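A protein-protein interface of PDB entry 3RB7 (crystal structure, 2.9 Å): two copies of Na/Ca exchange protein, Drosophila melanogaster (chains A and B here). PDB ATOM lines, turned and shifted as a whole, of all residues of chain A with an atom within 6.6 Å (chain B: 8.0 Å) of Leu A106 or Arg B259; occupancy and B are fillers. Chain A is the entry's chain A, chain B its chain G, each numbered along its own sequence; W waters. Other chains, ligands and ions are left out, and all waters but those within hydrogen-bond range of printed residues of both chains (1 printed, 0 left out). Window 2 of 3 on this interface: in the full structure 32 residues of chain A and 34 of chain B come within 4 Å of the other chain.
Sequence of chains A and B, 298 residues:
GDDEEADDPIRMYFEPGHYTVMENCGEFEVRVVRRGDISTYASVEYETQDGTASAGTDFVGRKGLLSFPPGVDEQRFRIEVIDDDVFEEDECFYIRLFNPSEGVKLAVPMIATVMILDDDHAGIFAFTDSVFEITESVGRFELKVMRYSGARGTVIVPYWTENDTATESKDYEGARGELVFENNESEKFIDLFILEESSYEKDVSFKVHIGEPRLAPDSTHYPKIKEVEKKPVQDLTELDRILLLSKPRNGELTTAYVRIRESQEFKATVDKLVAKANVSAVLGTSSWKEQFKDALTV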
ATOM      1  N   ILE A  10     -32.236   5.605 -12.550  1.00  0.00           N
ATOM      2  CA  ILE A  10     -30.974   5.281 -13.229  1.00  0.00           C
ATOM      3  C   ILE A  10     -31.132   4.098 -14.195  1.00  0.00           C
ATOM      4  O   ILE A  10     -31.418   4.317 -15.368  1.00  0.00           O
ATOM      5  CB  ILE A  10     -29.743   5.153 -12.228  1.00  0.00           C
ATOM      6  CG1 ILE A  10     -28.409   5.468 -12.925  1.00  0.00           C
ATOM      7  CG2 ILE A  10     -29.708   3.814 -11.484  1.00  0.00           C
ATOM      8  CD1 ILE A  10     -27.576   4.259 -13.278  1.00  0.00           C
ATOM      9  N   ARG A  11     -30.974   2.867 -13.708  1.00  0.00           N
ATOM     10  CA  ARG A  11     -31.170   1.661 -14.535  1.00  0.00           C
ATOM     11  C   ARG A  11     -32.424   0.839 -14.214  1.00  0.00           C
ATOM     12  O   ARG A  11     -33.212   1.194 -13.345  1.00  0.00           O
ATOM     13  CB  ARG A  11     -29.929   0.751 -14.530  1.00  0.00           C
ATOM     14  CG  ARG A  11     -29.231   0.623 -13.197  1.00  0.00           C
ATOM     15  CD  ARG A  11     -30.187   0.208 -12.115  1.00  0.00           C
ATOM     16  NE  ARG A  11     -30.014   1.035 -10.927  1.00  0.00           N
ATOM     17  CZ  ARG A  11     -29.205   0.745  -9.914  1.00  0.00           C
ATOM     18  NH1 ARG A  11     -28.480  -0.373  -9.930  1.00  0.00           N
ATOM     19  NH2 ARG A  11     -29.129   1.578  -8.880  1.00  0.00           N
ATOM     20  N   MET A  12     -32.586  -0.275 -14.925  1.00  0.00           N
ATOM     21  CA  MET A  12     -33.805  -1.095 -14.864  1.00  0.00           C
ATOM     22  C   MET A  12     -33.552  -2.538 -15.321  1.00  0.00           C
ATOM     23  O   MET A  12     -33.294  -2.770 -16.498  1.00  0.00           O
ATOM     24  CB  MET A  12     -34.884  -0.469 -15.750  1.00  0.00           C
ATOM     25  CG  MET A  12     -36.117  -1.318 -15.974  1.00  0.00           C
ATOM     26  SD  MET A  12     -37.250  -0.540 -17.147  1.00  0.00           S
ATOM     27  CE  MET A  12     -37.981   0.814 -16.224  1.00  0.00           C
ATOM     28  N   TYR A  13     -33.645  -3.505 -14.404  1.00  0.00           N
ATOM     29  CA  TYR A  13     -33.243  -4.885 -14.709  1.00  0.00           C
ATOM     30  C   TYR A  13     -34.219  -5.994 -14.283  1.00  0.00           C
ATOM     31  O   TYR A  13     -35.412  -5.759 -14.098  1.00  0.00           O
ATOM     32  CB  TYR A  13     -31.862  -5.161 -14.113  1.00  0.00           C
ATOM     33  CG  TYR A  13     -31.759  -4.797 -12.657  1.00  0.00           C
ATOM     34  CD1 TYR A  13     -31.985  -5.741 -11.662  1.00  0.00           C
ATOM     35  CD2 TYR A  13     -31.445  -3.505 -12.272  1.00  0.00           C
ATOM     36  CE1 TYR A  13     -31.896  -5.400 -10.318  1.00  0.00           C
ATOM     37  CE2 TYR A  13     -31.352  -3.155 -10.938  1.00  0.00           C
ATOM     38  CZ  TYR A  13     -31.578  -4.101  -9.967  1.00  0.00           C
ATOM     39  OH  TYR A  13     -31.481  -3.738  -8.646  1.00  0.00           O
ATOM     40  N   VAL A  44     -40.410   0.018 -20.232  1.00  0.00           N
ATOM     41  CA  VAL A  44     -39.518  -0.903 -20.919  1.00  0.00           C
ATOM     42  C   VAL A  44     -40.372  -2.017 -21.524  1.00  0.00           C
ATOM     43  O   VAL A  44     -41.563  -2.114 -21.216  1.00  0.00           O
ATOM     44  CB  VAL A  44     -38.476  -1.496 -19.952  1.00  0.00           C
ATOM     45  CG1 VAL A  44     -39.007  -2.765 -19.309  1.00  0.00           C
ATOM     46  CG2 VAL A  44     -37.164  -1.756 -20.667  1.00  0.00           C
ATOM     47  N   ARG A  96     -36.459 -11.390 -22.960  1.00  0.00           N
ATOM     48  CA  ARG A  96     -35.449 -10.375 -23.262  1.00  0.00           C
ATOM     49  C   ARG A  96     -35.964  -8.941 -23.160  1.00  0.00           C
ATOM     50  O   ARG A  96     -36.983  -8.584 -23.770  1.00  0.00           O
ATOM     51  CB  ARG A  96     -34.866 -10.614 -24.661  1.00  0.00           C
ATOM     52  CG  ARG A  96     -33.641  -9.780 -24.959  1.00  0.00           C
ATOM     53  CD  ARG A  96     -33.162  -9.906 -26.400  1.00  0.00           C
ATOM     54  NE  ARG A  96     -31.851  -9.275 -26.531  1.00  0.00           N
ATOM     55  CZ  ARG A  96     -31.643  -7.959 -26.459  1.00  0.00           C
ATOM     56  NH1 ARG A  96     -32.662  -7.123 -26.273  1.00  0.00           N
ATOM     57  NH2 ARG A  96     -30.414  -7.472 -26.576  1.00  0.00           N
ATOM     58  N   LEU A  97     -35.234  -8.126 -22.400  1.00  0.00           N
ATOM     59  CA  LEU A  97     -35.603  -6.732 -22.182  1.00  0.00           C
ATOM     60  C   LEU A  97     -35.057  -5.827 -23.275  1.00  0.00           C
ATOM     61  O   LEU A  97     -34.028  -6.116 -23.875  1.00  0.00           O
ATOM     62  CB  LEU A  97     -35.112  -6.244 -20.811  1.00  0.00           C
ATOM     63  CG  LEU A  97     -35.899  -6.676 -19.564  1.00  0.00           C
ATOM     64  CD1 LEU A  97     -35.160  -6.267 -18.295  1.00  0.00           C
ATOM     65  CD2 LEU A  97     -37.327  -6.127 -19.567  1.00  0.00           C
ATOM     66  N   PHE A  98     -35.751  -4.723 -23.525  1.00  0.00           N
ATOM     67  CA  PHE A  98     -35.318  -3.791 -24.551  1.00  0.00           C
ATOM     68  C   PHE A  98     -36.096  -2.475 -24.505  1.00  0.00           C
ATOM     69  O   PHE A  98     -37.101  -2.365 -23.808  1.00  0.00           O
ATOM     70  CB  PHE A  98     -35.429  -4.443 -25.936  1.00  0.00           C
ATOM     71  CG  PHE A  98     -36.844  -4.684 -26.393  1.00  0.00           C
ATOM     72  CD1 PHE A  98     -37.286  -5.966 -26.666  1.00  0.00           C
ATOM     73  CD2 PHE A  98     -37.731  -3.625 -26.557  1.00  0.00           C
ATOM     74  CE1 PHE A  98     -38.591  -6.185 -27.094  1.00  0.00           C
ATOM     75  CE2 PHE A  98     -39.030  -3.838 -26.978  1.00  0.00           C
ATOM     76  CZ  PHE A  98     -39.464  -5.117 -27.248  1.00  0.00           C
ATOM     77  N   ASN A  99     -35.621  -1.485 -25.254  1.00  0.00           N
ATOM     78  CA  ASN A  99     -36.320  -0.210 -25.400  1.00  0.00           C
ATOM     79  C   ASN A  99     -36.646   0.512 -24.093  1.00  0.00           C
ATOM     80  O   ASN A  99     -37.761   1.006 -23.916  1.00  0.00           O
ATOM     81  CB  ASN A  99     -37.604  -0.386 -26.221  1.00  0.00           C
ATOM     82  CG  ASN A  99     -37.342  -0.464 -27.719  1.00  0.00           C
ATOM     83  OD1 ASN A  99     -36.211  -0.297 -28.178  1.00  0.00           O
ATOM     84  ND2 ASN A  99     -38.398  -0.717 -28.490  1.00  0.00           N
ATOM     85  N   PRO A 100     -35.677   0.585 -23.170  1.00  0.00           N
ATOM     86  CA  PRO A 100     -35.947   1.377 -21.965  1.00  0.00           C
ATOM     87  C   PRO A 100     -36.092   2.873 -22.295  1.00  0.00           C
ATOM     88  O   PRO A 100     -35.261   3.416 -23.025  1.00  0.00           O
ATOM     89  CB  PRO A 100     -34.701   1.135 -21.100  1.00  0.00           C
ATOM     90  CG  PRO A 100     -34.062  -0.093 -21.653  1.00  0.00           C
ATOM     91  CD  PRO A 100     -34.374  -0.100 -23.109  1.00  0.00           C
ATOM     92  N   VAL A 104     -34.069   5.822 -18.180  1.00  0.00           N
ATOM     93  CA  VAL A 104     -33.637   4.527 -17.670  1.00  0.00           C
ATOM     94  C   VAL A 104     -32.770   3.720 -18.631  1.00  0.00           C
ATOM     95  O   VAL A 104     -33.135   3.476 -19.781  1.00  0.00           O
ATOM     96  CB  VAL A 104     -34.837   3.667 -17.246  1.00  0.00           C
ATOM     97  CG1 VAL A 104     -36.082   4.070 -18.014  1.00  0.00           C
ATOM     98  CG2 VAL A 104     -34.517   2.203 -17.452  1.00  0.00           C
ATOM     99  N   LYS A 105     -31.621   3.299 -18.124  1.00  0.00           N
ATOM    100  CA  LYS A 105     -30.661   2.507 -18.878  1.00  0.00           C
ATOM    101  C   LYS A 105     -30.830   1.019 -18.541  1.00  0.00           C
ATOM    102  O   LYS A 105     -31.634   0.658 -17.681  1.00  0.00           O
ATOM    103  CB  LYS A 105     -29.247   3.001 -18.550  1.00  0.00           C
ATOM    104  CG  LYS A 105     -29.113   3.521 -17.095  1.00  0.00           C
ATOM    105  CD  LYS A 105     -27.854   4.374 -16.836  1.00  0.00           C
ATOM    106  CE  LYS A 105     -28.158   5.868 -16.776  1.00  0.00           C
ATOM    107  NZ  LYS A 105     -27.107   6.567 -15.987  1.00  0.00           N
ATOM    108  N   LEU A 106     -30.076   0.160 -19.223  1.00  0.00           N
ATOM    109  CA  LEU A 106     -30.220  -1.288 -19.062  1.00  0.00           C
ATOM    110  C   LEU A 106     -29.043  -1.948 -18.354  1.00  0.00           C
ATOM    111  O   LEU A 106     -27.888  -1.836 -18.775  1.00  0.00           O
ATOM    112  CB  LEU A 106     -30.486  -1.970 -20.409  1.00  0.00           C
ATOM    113  CG  LEU A 106     -31.933  -2.430 -20.578  1.00  0.00           C
ATOM    114  CD1 LEU A 106     -32.212  -2.968 -21.971  1.00  0.00           C
ATOM    115  CD2 LEU A 106     -32.233  -3.475 -19.537  1.00  0.00           C
ATOM    116  N   ALA A 107     -29.357  -2.643 -17.271  1.00  0.00           N
ATOM    117  CA  ALA A 107     -28.339  -3.323 -16.497  1.00  0.00           C
ATOM    118  C   ALA A 107     -28.556  -4.824 -16.516  1.00  0.00           C
ATOM    119  O   ALA A 107     -29.498  -5.338 -17.128  1.00  0.00           O
ATOM    120  CB  ALA A 107     -28.325  -2.811 -15.070  1.00  0.00           C
ATOM    121  N   VAL A 108     -27.663  -5.519 -15.832  1.00  0.00           N
ATOM    122  CA  VAL A 108     -27.677  -6.965 -15.777  1.00  0.00           C
ATOM    123  C   VAL A 108     -28.723  -7.417 -14.769  1.00  0.00           C
ATOM    124  O   VAL A 108     -28.889  -6.777 -13.730  1.00  0.00           O
ATOM    125  CB  VAL A 108     -26.292  -7.461 -15.321  1.00  0.00           C
ATOM    126  CG1 VAL A 108     -26.166  -8.985 -15.458  1.00  0.00           C
ATOM    127  CG2 VAL A 108     -25.189  -6.715 -16.090  1.00  0.00           C
ATOM    128  N   PRO A 109     -29.465  -8.493 -15.085  1.00  0.00           N
ATOM    129  CA  PRO A 109     -29.565  -9.116 -16.409  1.00  0.00           C
ATOM    130  C   PRO A 109     -30.835  -8.664 -17.117  1.00  0.00           C
ATOM    131  O   PRO A 109     -31.894  -8.620 -16.501  1.00  0.00           O
ATOM    132  CB  PRO A 109     -29.698 -10.614 -16.084  1.00  0.00           C
ATOM    133  CG  PRO A 109     -29.659 -10.723 -14.567  1.00  0.00           C
ATOM    134  CD  PRO A 109     -30.013  -9.377 -14.047  1.00  0.00           C
ATOM    135  N   MET A 110     -30.751  -8.345 -18.398  1.00  0.00           N
ATOM    136  CA  MET A 110     -31.974  -8.058 -19.124  1.00  0.00           C
ATOM    137  C   MET A 110     -32.379  -9.219 -20.060  1.00  0.00           C
ATOM    138  O   MET A 110     -33.168  -9.046 -21.000  1.00  0.00           O
ATOM    139  CB  MET A 110     -31.881  -6.707 -19.838  1.00  0.00           C
ATOM    140  CG  MET A 110     -31.523  -6.759 -21.306  1.00  0.00           C
ATOM    141  SD  MET A 110     -29.895  -7.439 -21.633  1.00  0.00           S
ATOM    142  CE  MET A 110     -29.657  -6.843 -23.316  1.00  0.00           C
ATOM    143  N   ILE A 111     -31.836 -10.403 -19.779  1.00  0.00           N
ATOM    144  CA  ILE A 111     -32.255 -11.641 -20.435  1.00  0.00           C
ATOM    145  C   ILE A 111     -32.467 -12.712 -19.392  1.00  0.00           C
ATOM    146  O   ILE A 111     -31.534 -13.077 -18.672  1.00  0.00           O
ATOM    147  CB  ILE A 111     -31.200 -12.197 -21.403  1.00  0.00           C
ATOM    148  CG1 ILE A 111     -31.224 -11.445 -22.736  1.00  0.00           C
ATOM    149  CG2 ILE A 111     -31.448 -13.691 -21.639  1.00  0.00           C
ATOM    150  CD1 ILE A 111     -30.162 -11.905 -23.708  1.00  0.00           C
ATOM    151  N   VAL B 131     -26.008 -16.924 -19.570  1.00  0.00           N
ATOM    152  CA  VAL B 131     -25.654 -15.554 -19.962  1.00  0.00           C
ATOM    153  C   VAL B 131     -24.285 -15.098 -19.436  1.00  0.00           C
ATOM    154  O   VAL B 131     -24.021 -15.122 -18.223  1.00  0.00           O
ATOM    155  CB  VAL B 131     -26.689 -14.524 -19.494  1.00  0.00           C
ATOM    156  CG1 VAL B 131     -26.120 -13.123 -19.651  1.00  0.00           C
ATOM    157  CG2 VAL B 131     -27.981 -14.671 -20.275  1.00  0.00           C
ATOM    158  N   PHE B 132     -23.427 -14.668 -20.358  1.00  0.00           N
ATOM    159  CA  PHE B 132     -22.115 -14.141 -19.998  1.00  0.00           C
ATOM    160  C   PHE B 132     -21.998 -12.658 -20.321  1.00  0.00           C
ATOM    161  O   PHE B 132     -22.455 -12.201 -21.377  1.00  0.00           O
ATOM    162  CB  PHE B 132     -21.017 -14.887 -20.732  1.00  0.00           C
ATOM    163  CG  PHE B 132     -20.936 -16.329 -20.386  1.00  0.00           C
ATOM    164  CD1 PHE B 132     -19.882 -16.812 -19.626  1.00  0.00           C
ATOM    165  CD2 PHE B 132     -21.908 -17.209 -20.826  1.00  0.00           C
ATOM    166  CE1 PHE B 132     -19.792 -18.150 -19.309  1.00  0.00           C
ATOM    167  CE2 PHE B 132     -21.833 -18.551 -20.512  1.00  0.00           C
ATOM    168  CZ  PHE B 132     -20.770 -19.027 -19.749  1.00  0.00           C
ATOM    169  N   GLU B 133     -21.361 -11.922 -19.410  1.00  0.00           N
ATOM    170  CA  GLU B 133     -21.199 -10.481 -19.555  1.00  0.00           C
ATOM    171  C   GLU B 133     -19.793 -10.131 -20.028  1.00  0.00           C
ATOM    172  O   GLU B 133     -18.802 -10.728 -19.596  1.00  0.00           O
ATOM    173  CB  GLU B 133     -21.517  -9.779 -18.237  1.00  0.00           C
ATOM    174  CG  GLU B 133     -22.977  -9.914 -17.809  1.00  0.00           C
ATOM    175  CD  GLU B 133     -23.902  -9.018 -18.616  1.00  0.00           C
ATOM    176  OE1 GLU B 133     -23.413  -7.981 -19.112  1.00  0.00           O
ATOM    177  OE2 GLU B 133     -25.106  -9.343 -18.752  1.00  0.00           O
ATOM    178  N   ILE B 134     -19.712  -9.154 -20.917  1.00  0.00           N
ATOM    179  CA  ILE B 134     -18.464  -8.883 -21.605  1.00  0.00           C
ATOM    180  C   ILE B 134     -18.302  -7.384 -21.865  1.00  0.00           C
ATOM    181  O   ILE B 134     -19.211  -6.728 -22.391  1.00  0.00           O
ATOM    182  CB  ILE B 134     -18.402  -9.706 -22.900  1.00  0.00           C
ATOM    183  CG1 ILE B 134     -16.972 -10.109 -23.207  1.00  0.00           C
ATOM    184  CG2 ILE B 134     -19.032  -8.965 -24.056  1.00  0.00           C
ATOM    185  CD1 ILE B 134     -16.902 -11.200 -24.238  1.00  0.00           C
ATOM    186  N   THR B 135     -17.148  -6.841 -21.477  1.00  0.00           N
ATOM    187  CA  THR B 135     -17.004  -5.387 -21.381  1.00  0.00           C
ATOM    188  C   THR B 135     -16.583  -4.691 -22.676  1.00  0.00           C
ATOM    189  O   THR B 135     -15.755  -5.194 -23.437  1.00  0.00           O
ATOM    190  CB  THR B 135     -16.101  -4.944 -20.181  1.00  0.00           C
ATOM    191  OG1 THR B 135     -16.385  -3.582 -19.833  1.00  0.00           O
ATOM    192  CG2 THR B 135     -14.634  -5.073 -20.509  1.00  0.00           C
ATOM    193  N   GLU B 136     -17.206  -3.537 -22.906  1.00  0.00           N
ATOM    194  CA  GLU B 136     -16.917  -2.639 -24.024  1.00  0.00           C
ATOM    195  C   GLU B 136     -15.759  -3.079 -24.947  1.00  0.00           C
ATOM    196  O   GLU B 136     -15.946  -3.909 -25.850  1.00  0.00           O
ATOM    197  CB  GLU B 136     -16.699  -1.214 -23.480  1.00  0.00           C
ATOM    198  CG  GLU B 136     -16.495  -0.132 -24.527  1.00  0.00           C
ATOM    199  CD  GLU B 136     -17.234   1.138 -24.185  1.00  0.00           C
ATOM    200  OE1 GLU B 136     -16.578   2.117 -23.750  1.00  0.00           O
ATOM    201  OE2 GLU B 136     -18.477   1.139 -24.346  1.00  0.00           O
ATOM    202  N   ALA B 166     -26.311  -8.545 -31.989  1.00  0.00           N
ATOM    203  CA  ALA B 166     -24.928  -8.454 -32.418  1.00  0.00           C
ATOM    204  C   ALA B 166     -24.805  -9.266 -33.699  1.00  0.00           C
ATOM    205  O   ALA B 166     -25.273 -10.408 -33.766  1.00  0.00           O
ATOM    206  CB  ALA B 166     -24.005  -8.999 -31.352  1.00  0.00           C
ATOM    207  N   ILE B 194     -14.476 -10.291 -30.783  1.00  0.00           N
ATOM    208  CA  ILE B 194     -15.317  -9.087 -30.784  1.00  0.00           C
ATOM    209  C   ILE B 194     -14.546  -7.838 -31.241  1.00  0.00           C
ATOM    210  O   ILE B 194     -13.320  -7.840 -31.291  1.00  0.00           O
ATOM    211  CB  ILE B 194     -15.872  -8.791 -29.361  1.00  0.00           C
ATOM    212  CG1 ILE B 194     -16.040 -10.075 -28.553  1.00  0.00           C
ATOM    213  CG2 ILE B 194     -17.192  -8.026 -29.422  1.00  0.00           C
ATOM    214  CD1 ILE B 194     -16.893  -9.892 -27.331  1.00  0.00           C
ATOM    215  N   ASP B 203     -24.417  -2.401 -25.992  1.00  0.00           N
ATOM    216  CA  ASP B 203     -25.857  -2.567 -25.735  1.00  0.00           C
ATOM    217  C   ASP B 203     -26.434  -3.949 -26.091  1.00  0.00           C
ATOM    218  O   ASP B 203     -27.178  -4.523 -25.305  1.00  0.00           O
ATOM    219  CB  ASP B 203     -26.682  -1.445 -26.399  1.00  0.00           C
ATOM    220  CG  ASP B 203     -26.187  -1.089 -27.800  1.00  0.00           C
ATOM    221  OD1 ASP B 203     -26.698  -1.672 -28.789  1.00  0.00           O
ATOM    222  OD2 ASP B 203     -25.298  -0.210 -27.917  1.00  0.00           O
ATOM    223  N   VAL B 204     -26.082  -4.460 -27.270  1.00  0.00           N
ATOM    224  CA  VAL B 204     -26.670  -5.681 -27.826  1.00  0.00           C
ATOM    225  C   VAL B 204     -25.886  -6.961 -27.537  1.00  0.00           C
ATOM    226  O   VAL B 204     -24.943  -6.957 -26.735  1.00  0.00           O
ATOM    227  CB  VAL B 204     -26.866  -5.556 -29.338  1.00  0.00           C
ATOM    228  CG1 VAL B 204     -27.608  -4.271 -29.654  1.00  0.00           C
ATOM    229  CG2 VAL B 204     -25.512  -5.615 -30.062  1.00  0.00           C
ATOM    230  N   SER B 205     -26.265  -8.042 -28.226  1.00  0.00           N
ATOM    231  CA  SER B 205     -25.834  -9.396 -27.858  1.00  0.00           C
ATOM    232  C   SER B 205     -25.901 -10.449 -28.975  1.00  0.00           C
ATOM    233  O   SER B 205     -26.626 -10.297 -29.957  1.00  0.00           O
ATOM    234  CB  SER B 205     -26.684  -9.878 -26.681  1.00  0.00           C
ATOM    235  OG  SER B 205     -28.056  -9.564 -26.890  1.00  0.00           O
ATOM    236  N   PHE B 206     -25.130 -11.523 -28.804  1.00  0.00           N
ATOM    237  CA  PHE B 206     -25.235 -12.717 -29.651  1.00  0.00           C
ATOM    238  C   PHE B 206     -25.155 -14.004 -28.798  1.00  0.00           C
ATOM    239  O   PHE B 206     -24.639 -13.983 -27.669  1.00  0.00           O
ATOM    240  CB  PHE B 206     -24.168 -12.713 -30.765  1.00  0.00           C
ATOM    241  CG  PHE B 206     -22.743 -12.762 -30.255  1.00  0.00           C
ATOM    242  CD1 PHE B 206     -22.120 -11.618 -29.762  1.00  0.00           C
ATOM    243  CD2 PHE B 206     -22.024 -13.949 -30.272  1.00  0.00           C
ATOM    244  CE1 PHE B 206     -20.812 -11.660 -29.289  1.00  0.00           C
ATOM    245  CE2 PHE B 206     -20.716 -13.998 -29.799  1.00  0.00           C
ATOM    246  CZ  PHE B 206     -20.111 -12.848 -29.311  1.00  0.00           C
ATOM    247  N   LYS B 207     -25.682 -15.112 -29.318  1.00  0.00           N
ATOM    248  CA  LYS B 207     -25.589 -16.369 -28.586  1.00  0.00           C
ATOM    249  C   LYS B 207     -24.641 -17.362 -29.248  1.00  0.00           C
ATOM    250  O   LYS B 207     -24.465 -17.337 -30.463  1.00  0.00           O
ATOM    251  CB  LYS B 207     -26.976 -16.995 -28.293  1.00  0.00           C
ATOM    252  CG  LYS B 207     -28.042 -16.981 -29.406  1.00  0.00           C
ATOM    253  CD  LYS B 207     -29.397 -17.451 -28.827  1.00  0.00           C
ATOM    254  CE  LYS B 207     -30.518 -17.538 -29.865  1.00  0.00           C
ATOM    255  NZ  LYS B 207     -31.239 -16.255 -30.099  1.00  0.00           N
ATOM    256  N   ALA B 256     -25.263 -20.284 -24.839  1.00  0.00           N
ATOM    257  CA  ALA B 256     -24.818 -19.180 -24.008  1.00  0.00           C
ATOM    258  C   ALA B 256     -25.387 -17.885 -24.584  1.00  0.00           C
ATOM    259  O   ALA B 256     -26.107 -17.899 -25.582  1.00  0.00           O
ATOM    260  CB  ALA B 256     -23.295 -19.130 -23.945  1.00  0.00           C
ATOM    261  N   TYR B 257     -25.077 -16.774 -23.932  1.00  0.00           N
ATOM    262  CA  TYR B 257     -25.468 -15.455 -24.409  1.00  0.00           C
ATOM    263  C   TYR B 257     -24.349 -14.489 -24.017  1.00  0.00           C
ATOM    264  O   TYR B 257     -23.943 -14.458 -22.852  1.00  0.00           O
ATOM    265  CB  TYR B 257     -26.781 -15.018 -23.752  1.00  0.00           C
ATOM    266  CG  TYR B 257     -28.061 -15.307 -24.529  1.00  0.00           C
ATOM    267  CD1 TYR B 257     -28.858 -16.413 -24.226  1.00  0.00           C
ATOM    268  CD2 TYR B 257     -28.493 -14.449 -25.538  1.00  0.00           C
ATOM    269  CE1 TYR B 257     -30.039 -16.664 -24.923  1.00  0.00           C
ATOM    270  CE2 TYR B 257     -29.669 -14.697 -26.240  1.00  0.00           C
ATOM    271  CZ  TYR B 257     -30.437 -15.800 -25.929  1.00  0.00           C
ATOM    272  OH  TYR B 257     -31.598 -16.034 -26.630  1.00  0.00           O
ATOM    273  N   VAL B 258     -23.846 -13.710 -24.974  1.00  0.00           N
ATOM    274  CA  VAL B 258     -22.711 -12.811 -24.712  1.00  0.00           C
ATOM    275  C   VAL B 258     -23.081 -11.320 -24.787  1.00  0.00           C
ATOM    276  O   VAL B 258     -23.415 -10.816 -25.862  1.00  0.00           O
ATOM    277  CB  VAL B 258     -21.550 -13.102 -25.688  1.00  0.00           C
ATOM    278  CG1 VAL B 258     -20.462 -12.034 -25.574  1.00  0.00           C
ATOM    279  CG2 VAL B 258     -20.988 -14.497 -25.434  1.00  0.00           C
ATOM    280  N   ARG B 259     -22.999 -10.616 -23.654  1.00  0.00           N
ATOM    281  CA  ARG B 259     -23.486  -9.233 -23.561  1.00  0.00           C
ATOM    282  C   ARG B 259     -22.376  -8.178 -23.614  1.00  0.00           C
ATOM    283  O   ARG B 259     -21.433  -8.210 -22.820  1.00  0.00           O
ATOM    284  CB  ARG B 259     -24.308  -9.047 -22.283  1.00  0.00           C
ATOM    285  CG  ARG B 259     -24.607  -7.596 -21.898  1.00  0.00           C
ATOM    286  CD  ARG B 259     -26.088  -7.251 -22.033  1.00  0.00           C
ATOM    287  NE  ARG B 259     -26.429  -5.964 -21.421  1.00  0.00           N
ATOM    288  CZ  ARG B 259     -26.740  -5.805 -20.135  1.00  0.00           C
ATOM    289  NH1 ARG B 259     -26.742  -6.852 -19.312  1.00  0.00           N
ATOM    290  NH2 ARG B 259     -27.042  -4.596 -19.668  1.00  0.00           N
ATOM    291  N   ILE B 260     -22.527  -7.221 -24.530  1.00  0.00           N
ATOM    292  CA  ILE B 260     -21.491  -6.232 -24.823  1.00  0.00           C
ATOM    293  C   ILE B 260     -21.903  -4.807 -24.436  1.00  0.00           C
ATOM    294  O   ILE B 260     -21.158  -4.088 -23.760  1.00  0.00           O
ATOM    295  CB  ILE B 260     -21.133  -6.272 -26.326  1.00  0.00           C
ATOM    296  CG1 ILE B 260     -21.323  -7.693 -26.884  1.00  0.00           C
ATOM    297  CG2 ILE B 260     -19.714  -5.779 -26.556  1.00  0.00           C
ATOM    298  CD1 ILE B 260     -20.706  -7.926 -28.254  1.00  0.00           C
HETATM  299  O   HOH W   1     -25.129  -3.487 -16.960  1.00  0.00           O
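The guanidinium group (NH2) of Arg A96 lies within hydrogen-bond range of the side-chain hydroxyl (OG) of Ser B205, at 3.2 Å. The side-chain sulfur (SD) of Met A110 sits at hydrogen-bond distance from the guanidinium group (NE) of Arg B259 (3.8 Å). The backbone carbonyl oxygen (O) of Leu A106 is in hydrogen-bond range of the guanidinium group (NH2) of Arg B259 (3.0 Å).
The side-chain carboxylate (OE2) of Glu B133 lies within salt-bridge range of the guanidinium group (NH1) of Arg B259. The backbone NH of Phe B132 is in hydrogen-bond range of the backbone carbonyl oxygen of Tyr B257 (2.6 Å). N of Ile B134 lies within hydrogen-bond range of O of Arg B259 (2.7 Å). O of Phe B132 is in hydrogen-bond range of N of Arg B259 (2.8 Å). N of Leu A97 is in hydrogen-bond range of O of Met A110 (2.7 Å). The side-chain hydroxyl (OH) of Tyr B257 sits close to the side-chain amino group (NZ) of Lys B207 (3.5 Å).
Arg B259 touches Ala A107 (NH2 to C, 3.5 Å). Val A108 touches Glu B133 (CG1 to OE2, 3.5 Å). Arg B259 touches Val A108. Met A110 touches Asp B203 (CE to O, 3.9 Å). Val B131 touches Ile A111 (CG2 to CG2, 3.9 Å). Ile A111 touches Tyr B257.
Printed residues of chain B within 4 Å of Leu A106: Arg B259 (3.0 Å). Of chain A, only Leu A106 (3.0 Å), Ala A107 (3.5 Å), Val A108 (3.6 Å) and Met A110 (3.8 Å) come within 4 Å of Arg B259. Ala A107 touches one residue of chain B. Of the printed residues of chain B, Arg A96 touches Ser B205 (3.2 Å). Of the printed residues of chain B, Val A108 touches Glu B133 and Arg B259. Val A44 touches none of the printed residues of chain B. The nearest residue of chain B that does not touch Leu A106 is Asp B203 (6.2 Å). The nearest printed residue of chain B that does not touch Met A110 is Ser B205 (4.8 Å).
Of the 18 printed residues of chain B, 6 touch a printed residue of chain A. Among the printed residues, no Asp or Glu carboxylate lies within 4 Å of a Lys or Arg side-chain nitrogen of the other chain.
No position is printed for both chains.
Water W1 bridges the backbone NH of Val A108 (3.4 Å) and the guanidinium group of Arg B259 (3.5 Å).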
